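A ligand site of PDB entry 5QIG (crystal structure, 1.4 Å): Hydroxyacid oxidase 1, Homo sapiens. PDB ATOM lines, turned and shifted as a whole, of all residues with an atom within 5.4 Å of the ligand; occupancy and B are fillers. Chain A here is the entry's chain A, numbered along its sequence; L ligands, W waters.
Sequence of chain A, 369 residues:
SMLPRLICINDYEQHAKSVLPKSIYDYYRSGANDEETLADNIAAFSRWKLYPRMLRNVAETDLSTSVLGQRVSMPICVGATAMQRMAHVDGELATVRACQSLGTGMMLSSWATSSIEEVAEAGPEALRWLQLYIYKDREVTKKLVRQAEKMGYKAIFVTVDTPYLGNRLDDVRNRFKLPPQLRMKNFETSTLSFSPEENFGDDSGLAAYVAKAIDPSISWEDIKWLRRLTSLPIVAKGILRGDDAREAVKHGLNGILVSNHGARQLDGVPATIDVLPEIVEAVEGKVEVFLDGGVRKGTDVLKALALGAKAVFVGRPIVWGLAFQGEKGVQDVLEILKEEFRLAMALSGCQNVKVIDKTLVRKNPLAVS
O2 of the ligand lies within hydrogen-bond range of OG of Ser 109 (2.6 Å).
The backbone carbonyl oxygen of Ala 80 lies within hydrogen-bond range of an oxygen (O3) of the ligand, at 2.7 Å.
OG1 of Thr 159 lies within hydrogen-bond range of O1 of the ligand (2.7 Å).
The side-chain carboxylate (OD2) of Asp 292 lies within hydrogen-bond range of an oxygen (O4) of the ligand (2.8 Å).
NH2 of Arg 296 lies within salt-bridge range of O8 of the ligand, at 2.8 Å.
The backbone NH (N) of Gly 315 is in hydrogen-bond range of an oxygen (O7) of the ligand, at 2.8 Å.
NZ of Lys 237 lies within hydrogen-bond range of O1 of the ligand, 2.9 Å away.
N of Gly 294 is in hydrogen-bond range of O8 of the ligand (2.9 Å).
The backbone NH (N) of Arg 316 is in hydrogen-bond range of an oxygen (O9) of the ligand, at 3.0 Å.
An oxygen (O9) of the ligand is in salt-bridge range of the guanidinium group (NH1) of Arg 316 (3.0 Å).
The side-chain amide oxygen of Gln 131 is in hydrogen-bond range of a nitrogen (N2) of the ligand (3.0 Å).
A nitrogen (N3) of the ligand is in hydrogen-bond range of the backbone NH (N) of Ala 82.
OH of Tyr 133 lies within hydrogen-bond range of N2 of the ligand, at 3.3 Å.
An oxygen (O4) of the ligand sits at hydrogen-bond distance from the side-chain hydroxyl (OG) of Ser 259, at 3.3 Å.
The backbone NH (N) of Gly 293 sits close to an oxygen (O6) of the ligand, 3.5 Å away.
NE2 of His 261 sits at hydrogen-bond distance from N1 of the ligand.
The side-chain hydroxyl (OG) of Ser 109 is in hydrogen-bond range of the backbone NH (N) of Trp 111 (2.8 Å).
The side-chain sulfur (SD) of Met 107 lies within hydrogen-bond range of the backbone NH (N) of Ala 80, 3.6 Å away.
The side-chain carboxylate of Asp 292 lies within hydrogen-bond range of the side-chain hydroxyl of Ser 259 (2.7 Å).
The guanidinium group (NE) of Arg 316 is in hydrogen-bond range of the backbone carbonyl oxygen (O) of Tyr 28.
The backbone carbonyl oxygen of Gln 131 lies within hydrogen-bond range of the side-chain hydroxyl of Ser 110, at 2.6 Å.
The side-chain hydroxyl (OG) of Ser 259 is in hydrogen-bond range of the backbone NH (N) of His 261, at 3.0 Å.
The backbone carbonyl oxygen (O) of Tyr 28 is in hydrogen-bond range of the guanidinium group (NH1) of Arg 264 (3.4 Å).
NH1 of Arg 264 lies within hydrogen-bond range of O of Tyr 27 (2.8 Å).
Tyr 27 touches the ligand.
CD1 of Tyr 28 touches C7 of the ligand, 3.4 Å away.
Thr 81 touches the ligand (CA to C4, 3.5 Å).
Trp 111 touches the ligand (CE3 to O2, 3.8 Å).
Gly 262 touches the ligand (CA to O6, 3.5 Å).
Arg 264 touches the ligand (NH2 to C7, 3.4 Å).
Val 314 touches the ligand.
Hydrophobic or aromatic side chains that line the ligand: Tyr 27, Tyr 28, Ala 82, Trp 111, Tyr 133 and His 261.
22 residues have an atom within 4 Å of the ligand: Tyr 27, Tyr 28, Ala 80, Thr 81, Ala 82, Ser 109, Trp 111, Gln 131, Tyr 133, Thr 159, Lys 237, Ser 259, His 261, Gly 262, Arg 264, Asp 292, Gly 293, Gly 294, Arg 296, Val 314, Gly 315 and Arg 316.
Water W3 lies within hydrogen-bond range of an oxygen (O8) of the ligand (2.8 Å), the side-chain amide nitrogen of Asn 41 (2.9 Å) and the guanidinium group of Arg 316 (3.1 Å).
Water W1 lies within hydrogen-bond range of OD2 of Asp 292 (2.8 Å) and O3 of the ligand (3.0 Å).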
ATOM      1  N   TYR A  27      28.194 -23.154 -12.019  1.00  0.00           N
ATOM      2  CA  TYR A  27      27.787 -24.277 -11.184  1.00  0.00           C
ATOM      3  C   TYR A  27      26.293 -24.220 -10.909  1.00  0.00           C
ATOM      4  O   TYR A  27      25.581 -25.216 -11.006  1.00  0.00           O
ATOM      5  CB  TYR A  27      28.611 -24.353  -9.865  1.00  0.00           C
ATOM      6  CG  TYR A  27      27.956 -25.252  -8.837  1.00  0.00           C
ATOM      7  CD1 TYR A  27      27.985 -26.622  -8.973  1.00  0.00           C
ATOM      8  CD2 TYR A  27      27.202 -24.718  -7.789  1.00  0.00           C
ATOM      9  CE1 TYR A  27      27.305 -27.449  -8.097  1.00  0.00           C
ATOM     10  CE2 TYR A  27      26.520 -25.527  -6.915  1.00  0.00           C
ATOM     11  CZ  TYR A  27      26.580 -26.915  -7.041  1.00  0.00           C
ATOM     12  OH  TYR A  27      25.886 -27.772  -6.212  1.00  0.00           O
ATOM     13  N   TYR A  28      25.806 -23.053 -10.523  1.00  0.00           N
ATOM     14  CA  TYR A  28      24.414 -22.908 -10.131  1.00  0.00           C
ATOM     15  C   TYR A  28      23.481 -23.017 -11.372  1.00  0.00           C
ATOM     16  O   TYR A  28      22.370 -23.579 -11.277  1.00  0.00           O
ATOM     17  CB  TYR A  28      24.205 -21.576  -9.408  1.00  0.00           C
ATOM     18  CG  TYR A  28      24.793 -21.433  -8.009  1.00  0.00           C
ATOM     19  CD1 TYR A  28      24.599 -22.410  -7.065  1.00  0.00           C
ATOM     20  CD2 TYR A  28      25.446 -20.260  -7.614  1.00  0.00           C
ATOM     21  CE1 TYR A  28      25.075 -22.258  -5.736  1.00  0.00           C
ATOM     22  CE2 TYR A  28      25.913 -20.071  -6.310  1.00  0.00           C
ATOM     23  CZ  TYR A  28      25.721 -21.078  -5.385  1.00  0.00           C
ATOM     24  OH  TYR A  28      26.153 -20.854  -4.079  1.00  0.00           O
ATOM     25  N   ASN A  41      12.294 -27.612 -18.989  1.00  0.00           N
ATOM     26  CA  ASN A  41      11.608 -27.377 -17.722  1.00  0.00           C
ATOM     27  C   ASN A  41      10.882 -26.047 -17.733  1.00  0.00           C
ATOM     28  O   ASN A  41       9.811 -25.947 -17.159  1.00  0.00           O
ATOM     29  CB  ASN A  41      12.562 -27.393 -16.523  1.00  0.00           C
ATOM     30  CG  ASN A  41      12.852 -28.775 -15.999  1.00  0.00           C
ATOM     31  OD1 ASN A  41      12.217 -29.754 -16.414  1.00  0.00           O
ATOM     32  ND2 ASN A  41      13.887 -28.877 -15.101  1.00  0.00           N
ATOM     33  N   GLY A  79      13.645 -25.410  -2.207  1.00  0.00           N
ATOM     34  CA  GLY A  79      14.270 -26.682  -2.477  1.00  0.00           C
ATOM     35  C   GLY A  79      15.738 -26.715  -2.094  1.00  0.00           C
ATOM     36  O   GLY A  79      16.392 -25.673  -1.976  1.00  0.00           O
ATOM     37  N   ALA A  80      16.274 -27.926  -1.904  1.00  0.00           N
ATOM     38  CA  ALA A  80      17.696 -28.129  -1.561  1.00  0.00           C
ATOM     39  C   ALA A  80      18.638 -27.672  -2.692  1.00  0.00           C
ATOM     40  O   ALA A  80      18.508 -28.124  -3.839  1.00  0.00           O
ATOM     41  CB  ALA A  80      17.950 -29.586  -1.223  1.00  0.00           C
ATOM     42  N   THR A  81      19.504 -26.721  -2.378  1.00  0.00           N
ATOM     43  CA  THR A  81      20.562 -26.328  -3.305  1.00  0.00           C
ATOM     44  C   THR A  81      21.841 -26.285  -2.511  1.00  0.00           C
ATOM     45  O   THR A  81      21.934 -25.559  -1.488  1.00  0.00           O
ATOM     46  CB  THR A  81      20.319 -24.975  -4.002  1.00  0.00           C
ATOM     47  OG1 THR A  81      19.917 -24.018  -3.048  1.00  0.00           O
ATOM     48  CG2 THR A  81      19.217 -25.071  -5.045  1.00  0.00           C
ATOM     49  N   ALA A  82      22.805 -27.097  -2.935  1.00  0.00           N
ATOM     50  CA  ALA A  82      24.042 -27.217  -2.219  1.00  0.00           C
ATOM     51  C   ALA A  82      24.860 -25.914  -2.108  1.00  0.00           C
ATOM     52  O   ALA A  82      24.811 -25.041  -2.951  1.00  0.00           O
ATOM     53  CB  ALA A  82      24.890 -28.296  -2.862  1.00  0.00           C
ATOM     54  N   MET A 107      13.906 -26.879   2.539  1.00  0.00           N
ATOM     55  CA  MET A 107      14.559 -28.172   2.409  1.00  0.00           C
ATOM     56  C   MET A 107      16.097 -27.956   2.398  1.00  0.00           C
ATOM     57  O   MET A 107      16.649 -27.285   1.525  1.00  0.00           O
ATOM     58  CB  MET A 107      14.095 -28.862   1.137  1.00  0.00           C
ATOM     59  CG  MET A 107      14.622 -30.285   0.972  1.00  0.00           C
ATOM     60  SD  MET A 107      14.570 -30.895  -0.730  1.00  0.00           S
ATOM     61  CE  MET A 107      12.860 -30.588  -1.154  1.00  0.00           C
ATOM     62  N   SER A 109      19.952 -29.001   2.058  1.00  0.00           N
ATOM     63  CA  SER A 109      20.825 -29.922   1.371  1.00  0.00           C
ATOM     64  C   SER A 109      21.714 -30.688   2.326  1.00  0.00           C
ATOM     65  O   SER A 109      22.311 -30.085   3.214  1.00  0.00           O
ATOM     66  CB  SER A 109      21.721 -29.137   0.395  1.00  0.00           C
ATOM     67  OG  SER A 109      22.693 -29.985  -0.246  1.00  0.00           O
ATOM     68  N   SER A 110      21.934 -31.961   2.053  1.00  0.00           N
ATOM     69  CA  SER A 110      23.012 -32.722   2.746  1.00  0.00           C
ATOM     70  C   SER A 110      24.383 -32.080   2.475  1.00  0.00           C
ATOM     71  O   SER A 110      25.321 -32.276   3.251  1.00  0.00           O
ATOM     72  CB  SER A 110      22.998 -34.211   2.299  1.00  0.00           C
ATOM     73  OG  SER A 110      22.031 -34.924   3.023  1.00  0.00           O
ATOM     74  N   TRP A 111      24.525 -31.391   1.354  1.00  0.00           N
ATOM     75  CA  TRP A 111      25.777 -30.721   0.927  1.00  0.00           C
ATOM     76  C   TRP A 111      25.791 -29.215   1.214  1.00  0.00           C
ATOM     77  O   TRP A 111      26.392 -28.440   0.511  1.00  0.00           O
ATOM     78  CB  TRP A 111      26.012 -30.940  -0.591  1.00  0.00           C
ATOM     79  CG  TRP A 111      26.126 -32.372  -1.031  1.00  0.00           C
ATOM     80  CD1 TRP A 111      26.405 -33.454  -0.233  1.00  0.00           C
ATOM     81  CD2 TRP A 111      26.028 -32.884  -2.383  1.00  0.00           C
ATOM     82  NE1 TRP A 111      26.461 -34.604  -0.997  1.00  0.00           N
ATOM     83  CE2 TRP A 111      26.216 -34.276  -2.317  1.00  0.00           C
ATOM     84  CE3 TRP A 111      25.711 -32.306  -3.626  1.00  0.00           C
ATOM     85  CZ2 TRP A 111      26.145 -35.090  -3.465  1.00  0.00           C
ATOM     86  CZ3 TRP A 111      25.666 -33.130  -4.743  1.00  0.00           C
ATOM     87  CH2 TRP A 111      25.872 -34.481  -4.653  1.00  0.00           C
ATOM     88  N   GLN A 131      17.111 -32.788   3.126  1.00  0.00           N
ATOM     89  CA  GLN A 131      17.372 -33.602   1.922  1.00  0.00           C
ATOM     90  C   GLN A 131      18.572 -34.512   2.217  1.00  0.00           C
ATOM     91  O   GLN A 131      19.616 -34.035   2.654  1.00  0.00           O
ATOM     92  CB  GLN A 131      17.671 -32.719   0.738  1.00  0.00           C
ATOM     93  CG  GLN A 131      18.066 -33.458  -0.518  1.00  0.00           C
ATOM     94  CD  GLN A 131      19.550 -33.791  -0.564  1.00  0.00           C
ATOM     95  OE1 GLN A 131      20.390 -32.890  -0.352  1.00  0.00           O
ATOM     96  NE2 GLN A 131      19.883 -35.057  -0.940  1.00  0.00           N
ATOM     97  N   TYR A 133      21.186 -37.645   1.048  1.00  0.00           N
ATOM     98  CA  TYR A 133      21.850 -38.594   0.162  1.00  0.00           C
ATOM     99  C   TYR A 133      22.226 -39.817   0.979  1.00  0.00           C
ATOM    100  O   TYR A 133      22.607 -39.691   2.157  1.00  0.00           O
ATOM    101  CB  TYR A 133      23.111 -37.958  -0.419  1.00  0.00           C
ATOM    102  CG  TYR A 133      22.850 -37.001  -1.566  1.00  0.00           C
ATOM    103  CD1 TYR A 133      22.272 -37.468  -2.723  1.00  0.00           C
ATOM    104  CD2 TYR A 133      23.167 -35.660  -1.496  1.00  0.00           C
ATOM    105  CE1 TYR A 133      22.046 -36.641  -3.769  1.00  0.00           C
ATOM    106  CE2 TYR A 133      22.938 -34.788  -2.553  1.00  0.00           C
ATOM    107  CZ  TYR A 133      22.402 -35.311  -3.703  1.00  0.00           C
ATOM    108  OH  TYR A 133      22.135 -34.531  -4.789  1.00  0.00           O
ATOM    109  N   THR A 159      16.987 -38.285  -1.950  1.00  0.00           N
ATOM    110  CA  THR A 159      17.257 -38.075  -3.370  1.00  0.00           C
ATOM    111  C   THR A 159      17.594 -39.429  -3.950  1.00  0.00           C
ATOM    112  O   THR A 159      18.498 -40.124  -3.478  1.00  0.00           O
ATOM    113  CB  THR A 159      18.348 -37.040  -3.567  1.00  0.00           C
ATOM    114  OG1 THR A 159      17.895 -35.810  -2.986  1.00  0.00           O
ATOM    115  CG2 THR A 159      18.655 -36.843  -5.054  1.00  0.00           C
ATOM    116  N   LYS A 237      12.538 -38.106  -3.723  1.00  0.00           N
ATOM    117  CA  LYS A 237      12.834 -36.957  -4.580  1.00  0.00           C
ATOM    118  C   LYS A 237      13.598 -37.399  -5.815  1.00  0.00           C
ATOM    119  O   LYS A 237      14.682 -37.972  -5.704  1.00  0.00           O
ATOM    120  CB  LYS A 237      13.633 -35.935  -3.763  1.00  0.00           C
ATOM    121  CG  LYS A 237      14.188 -34.761  -4.569  1.00  0.00           C
ATOM    122  CD  LYS A 237      14.978 -33.770  -3.700  1.00  0.00           C
ATOM    123  CE  LYS A 237      15.434 -32.534  -4.438  1.00  0.00           C
ATOM    124  NZ  LYS A 237      16.499 -32.837  -5.389  1.00  0.00           N
ATOM    125  N   SER A 259      10.777 -34.603  -9.923  1.00  0.00           N
ATOM    126  CA  SER A 259      11.961 -33.803 -10.047  1.00  0.00           C
ATOM    127  C   SER A 259      12.883 -34.492 -11.035  1.00  0.00           C
ATOM    128  O   SER A 259      12.995 -35.710 -11.035  1.00  0.00           O
ATOM    129  CB  SER A 259      12.662 -33.665  -8.692  1.00  0.00           C
ATOM    130  OG  SER A 259      13.855 -32.945  -8.801  1.00  0.00           O
ATOM    131  N   HIS A 261      15.942 -33.119 -10.930  1.00  0.00           N
ATOM    132  CA  HIS A 261      17.110 -32.557 -10.275  1.00  0.00           C
ATOM    133  C   HIS A 261      17.559 -31.238 -10.951  1.00  0.00           C
ATOM    134  O   HIS A 261      18.734 -30.994 -11.181  1.00  0.00           O
ATOM    135  CB  HIS A 261      18.248 -33.620 -10.259  1.00  0.00           C
ATOM    136  CG  HIS A 261      19.256 -33.469  -9.169  1.00  0.00           C
ATOM    137  ND1 HIS A 261      19.505 -34.485  -8.266  1.00  0.00           N
ATOM    138  CD2 HIS A 261      20.148 -32.488  -8.892  1.00  0.00           C
ATOM    139  CE1 HIS A 261      20.479 -34.101  -7.451  1.00  0.00           C
ATOM    140  NE2 HIS A 261      20.900 -32.893  -7.825  1.00  0.00           N
ATOM    141  N   GLY A 262      16.586 -30.391 -11.286  1.00  0.00           N
ATOM    142  CA  GLY A 262      16.852 -29.144 -11.970  1.00  0.00           C
ATOM    143  C   GLY A 262      17.584 -29.373 -13.300  1.00  0.00           C
ATOM    144  O   GLY A 262      18.362 -28.564 -13.743  1.00  0.00           O
ATOM    145  N   ARG A 264      19.852 -31.479 -13.997  1.00  0.00           N
ATOM    146  CA  ARG A 264      21.311 -31.611 -13.753  1.00  0.00           C
ATOM    147  C   ARG A 264      21.821 -33.036 -13.755  1.00  0.00           C
ATOM    148  O   ARG A 264      23.031 -33.248 -13.599  1.00  0.00           O
ATOM    149  CB  ARG A 264      21.668 -30.937 -12.428  1.00  0.00           C
ATOM    150  CG  ARG A 264      21.401 -29.447 -12.457  1.00  0.00           C
ATOM    151  CD  ARG A 264      21.305 -28.837 -11.103  1.00  0.00           C
ATOM    152  NE  ARG A 264      22.508 -28.761 -10.324  1.00  0.00           N
ATOM    153  CZ  ARG A 264      23.377 -27.764 -10.384  1.00  0.00           C
ATOM    154  NH1 ARG A 264      23.281 -26.835 -11.335  1.00  0.00           N
ATOM    155  NH2 ARG A 264      24.357 -27.681  -9.494  1.00  0.00           N
ATOM    156  N   ASP A 292       9.319 -29.864  -8.589  1.00  0.00           N
ATOM    157  CA  ASP A 292      10.330 -28.820  -8.798  1.00  0.00           C
ATOM    158  C   ASP A 292      10.828 -28.887 -10.234  1.00  0.00           C
ATOM    159  O   ASP A 292      10.547 -29.861 -10.947  1.00  0.00           O
ATOM    160  CB  ASP A 292      11.450 -28.843  -7.741  1.00  0.00           C
ATOM    161  CG  ASP A 292      12.373 -30.020  -7.800  1.00  0.00           C
ATOM    162  OD1 ASP A 292      12.524 -30.612  -8.869  1.00  0.00           O
ATOM    163  OD2 ASP A 292      13.000 -30.312  -6.751  1.00  0.00           O
ATOM    164  N   GLY A 293      11.561 -27.859 -10.660  1.00  0.00           N
ATOM    165  CA  GLY A 293      12.173 -27.807 -11.983  1.00  0.00           C
ATOM    166  C   GLY A 293      11.454 -26.780 -12.859  1.00  0.00           C
ATOM    167  O   GLY A 293      10.385 -27.035 -13.379  1.00  0.00           O
ATOM    168  N   GLY A 294      12.070 -25.613 -12.985  1.00  0.00           N
ATOM    169  CA  GLY A 294      11.605 -24.590 -13.885  1.00  0.00           C
ATOM    170  C   GLY A 294      10.598 -23.612 -13.330  1.00  0.00           C
ATOM    171  O   GLY A 294      10.068 -22.801 -14.089  1.00  0.00           O
ATOM    172  N   VAL A 295      10.300 -23.686 -12.026  1.00  0.00           N
ATOM    173  CA  VAL A 295       9.357 -22.728 -11.431  1.00  0.00           C
ATOM    174  C   VAL A 295      10.040 -21.357 -11.305  1.00  0.00           C
ATOM    175  O   VAL A 295      11.004 -21.180 -10.547  1.00  0.00           O
ATOM    176  CB  VAL A 295       8.805 -23.226 -10.079  1.00  0.00           C
ATOM    177  CG1 VAL A 295       7.893 -22.183  -9.456  1.00  0.00           C
ATOM    178  CG2 VAL A 295       8.092 -24.554 -10.239  1.00  0.00           C
ATOM    179  N   ARG A 296       9.461 -20.378 -12.020  1.00  0.00           N
ATOM    180  CA  ARG A 296       9.957 -19.025 -12.050  1.00  0.00           C
ATOM    181  C   ARG A 296       8.907 -17.951 -11.843  1.00  0.00           C
ATOM    182  O   ARG A 296       9.264 -16.811 -11.586  1.00  0.00           O
ATOM    183  CB  ARG A 296      10.675 -18.736 -13.358  1.00  0.00           C
ATOM    184  CG  ARG A 296      11.785 -19.684 -13.790  1.00  0.00           C
ATOM    185  CD  ARG A 296      12.991 -19.647 -12.892  1.00  0.00           C
ATOM    186  NE  ARG A 296      14.025 -20.642 -13.266  1.00  0.00           N
ATOM    187  CZ  ARG A 296      14.224 -21.811 -12.647  1.00  0.00           C
ATOM    188  NH1 ARG A 296      13.488 -22.197 -11.600  1.00  0.00           N
ATOM    189  NH2 ARG A 296      15.183 -22.618 -13.080  1.00  0.00           N
ATOM    190  N   PHE A 313       8.629 -26.618  -5.224  1.00  0.00           N
ATOM    191  CA  PHE A 313       9.894 -26.202  -4.642  1.00  0.00           C
ATOM    192  C   PHE A 313      10.656 -25.414  -5.717  1.00  0.00           C
ATOM    193  O   PHE A 313      10.610 -25.740  -6.908  1.00  0.00           O
ATOM    194  CB  PHE A 313      10.716 -27.415  -4.161  1.00  0.00           C
ATOM    195  CG  PHE A 313      10.088 -28.121  -3.018  1.00  0.00           C
ATOM    196  CD1 PHE A 313      10.463 -27.853  -1.719  1.00  0.00           C
ATOM    197  CD2 PHE A 313       9.086 -29.042  -3.235  1.00  0.00           C
ATOM    198  CE1 PHE A 313       9.844 -28.499  -0.639  1.00  0.00           C
ATOM    199  CE2 PHE A 313       8.454 -29.661  -2.158  1.00  0.00           C
ATOM    200  CZ  PHE A 313       8.837 -29.388  -0.874  1.00  0.00           C
ATOM    201  N   VAL A 314      11.350 -24.377  -5.241  1.00  0.00           N
ATOM    202  CA  VAL A 314      12.220 -23.556  -6.066  1.00  0.00           C
ATOM    203  C   VAL A 314      13.649 -23.735  -5.676  1.00  0.00           C
ATOM    204  O   VAL A 314      14.011 -23.718  -4.494  1.00  0.00           O
ATOM    205  CB  VAL A 314      11.851 -22.049  -6.116  1.00  0.00           C
ATOM    206  CG1 VAL A 314      10.546 -21.880  -6.919  1.00  0.00           C
ATOM    207  CG2 VAL A 314      11.719 -21.474  -4.760  1.00  0.00           C
ATOM    208  N   GLY A 315      14.477 -23.942  -6.691  1.00  0.00           N
ATOM    209  CA  GLY A 315      15.934 -24.105  -6.501  1.00  0.00           C
ATOM    210  C   GLY A 315      16.689 -22.849  -6.815  1.00  0.00           C
ATOM    211  O   GLY A 315      16.976 -22.043  -5.941  1.00  0.00           O
ATOM    212  N   ARG A 316      17.048 -22.677  -8.077  1.00  0.00           N
ATOM    213  CA  ARG A 316      17.947 -21.602  -8.486  1.00  0.00           C
ATOM    214  C   ARG A 316      17.479 -20.197  -8.095  1.00  0.00           C
ATOM    215  O   ARG A 316      18.303 -19.410  -7.665  1.00  0.00           O
ATOM    216  CB  ARG A 316      18.178 -21.642  -9.980  1.00  0.00           C
ATOM    217  CG  ARG A 316      18.964 -22.861 -10.419  1.00  0.00           C
ATOM    218  CD  ARG A 316      19.136 -22.926 -11.892  1.00  0.00           C
ATOM    219  NE  ARG A 316      19.838 -24.131 -12.350  1.00  0.00           N
ATOM    220  CZ  ARG A 316      19.257 -25.276 -12.695  1.00  0.00           C
ATOM    221  NH1 ARG A 316      17.948 -25.445 -12.551  1.00  0.00           N
ATOM    222  NH2 ARG A 316      19.989 -26.245 -13.249  1.00  0.00           N
ATOM    223  N   PRO A 317      16.152 -19.915  -8.143  1.00  0.00           N
ATOM    224  CA  PRO A 317      15.761 -18.532  -7.747  1.00  0.00           C
ATOM    225  C   PRO A 317      16.232 -18.126  -6.352  1.00  0.00           C
ATOM    226  O   PRO A 317      16.552 -16.965  -6.113  1.00  0.00           O
ATOM    227  CB  PRO A 317      14.257 -18.547  -7.877  1.00  0.00           C
ATOM    228  CG  PRO A 317      14.008 -19.563  -9.004  1.00  0.00           C
ATOM    229  CD  PRO A 317      15.006 -20.654  -8.728  1.00  0.00           C
ATOM    230  N   VAL A 319      19.005 -19.124  -4.817  1.00  0.00           N
ATOM    231  CA  VAL A 319      20.438 -18.809  -4.942  1.00  0.00           C
ATOM    232  C   VAL A 319      20.634 -17.427  -5.537  1.00  0.00           C
ATOM    233  O   VAL A 319      21.495 -16.675  -5.059  1.00  0.00           O
ATOM    234  CB  VAL A 319      21.170 -19.881  -5.769  1.00  0.00           C
ATOM    235  CG1 VAL A 319      22.613 -19.492  -5.938  1.00  0.00           C
ATOM    236  CG2 VAL A 319      21.033 -21.215  -5.056  1.00  0.00           C
HETATM  237  N1  LIG L   1      19.178 -31.635  -5.062  1.00  0.00           N
HETATM  238  C1  LIG L   1      19.522 -32.381  -3.991  1.00  0.00           C
HETATM  239  O1  LIG L   1      18.822 -33.354  -3.748  1.00  0.00           O
HETATM  240  N2  LIG L   1      20.569 -32.058  -3.203  1.00  0.00           N
HETATM  241  C2  LIG L   1      21.381 -31.029  -3.468  1.00  0.00           C
HETATM  242  O2  LIG L   1      22.337 -30.746  -2.751  1.00  0.00           O
HETATM  243  C3  LIG L   1      21.109 -30.205  -4.630  1.00  0.00           C
HETATM  244  N3  LIG L   1      21.897 -29.154  -4.934  1.00  0.00           N
HETATM  245  C4  LIG L   1      21.605 -28.331  -5.968  1.00  0.00           C
HETATM  246  C5  LIG L   1      22.405 -27.221  -6.286  1.00  0.00           C
HETATM  247  C6  LIG L   1      22.012 -26.409  -7.331  1.00  0.00           C
HETATM  248  C7  LIG L   1      22.854 -25.229  -7.661  1.00  0.00           C
HETATM  249  C8  LIG L   1      20.835 -26.715  -8.149  1.00  0.00           C
HETATM  250  C9  LIG L   1      20.457 -25.782  -9.291  1.00  0.00           C
HETATM  251  C10 LIG L   1      20.030 -27.776  -7.815  1.00  0.00           C
HETATM  252  C11 LIG L   1      20.399 -28.635  -6.781  1.00  0.00           C
HETATM  253  N4  LIG L   1      19.597 -29.757  -6.469  1.00  0.00           N
HETATM  254  C12 LIG L   1      19.921 -30.538  -5.367  1.00  0.00           C
HETATM  255  C13 LIG L   1      18.334 -30.040  -7.172  1.00  0.00           C
HETATM  256  C14 LIG L   1      17.258 -29.085  -6.526  1.00  0.00           C
HETATM  257  O3  LIG L   1      16.817 -29.644  -5.233  1.00  0.00           O
HETATM  258  C15 LIG L   1      15.988 -28.952  -7.331  1.00  0.00           C
HETATM  259  O4  LIG L   1      15.560 -30.259  -7.766  1.00  0.00           O
HETATM  260  C16 LIG L   1      16.103 -28.054  -8.540  1.00  0.00           C
HETATM  261  O5  LIG L   1      16.951 -26.941  -8.229  1.00  0.00           O
HETATM  262  C17 LIG L   1      14.783 -27.548  -9.010  1.00  0.00           C
HETATM  263  O6  LIG L   1      14.871 -26.839 -10.242  1.00  0.00           O
HETATM  264  P1  LIG L   1      15.019 -25.219 -10.331  1.00  0.00           P
HETATM  265  O7  LIG L   1      14.073 -24.509  -9.382  1.00  0.00           O
HETATM  266  O8  LIG L   1      14.657 -25.010 -11.800  1.00  0.00           O
HETATM  267  O9  LIG L   1      16.422 -24.846 -10.008  1.00  0.00           O
HETATM  268  O   HOH W   1      14.027 -29.283  -4.345  1.00  0.00           O
HETATM  269  O   HOH W   2      11.479 -25.287  -9.566  1.00  0.00           O
HETATM  270  O   HOH W   3      15.388 -26.674 -13.888  1.00  0.00           O
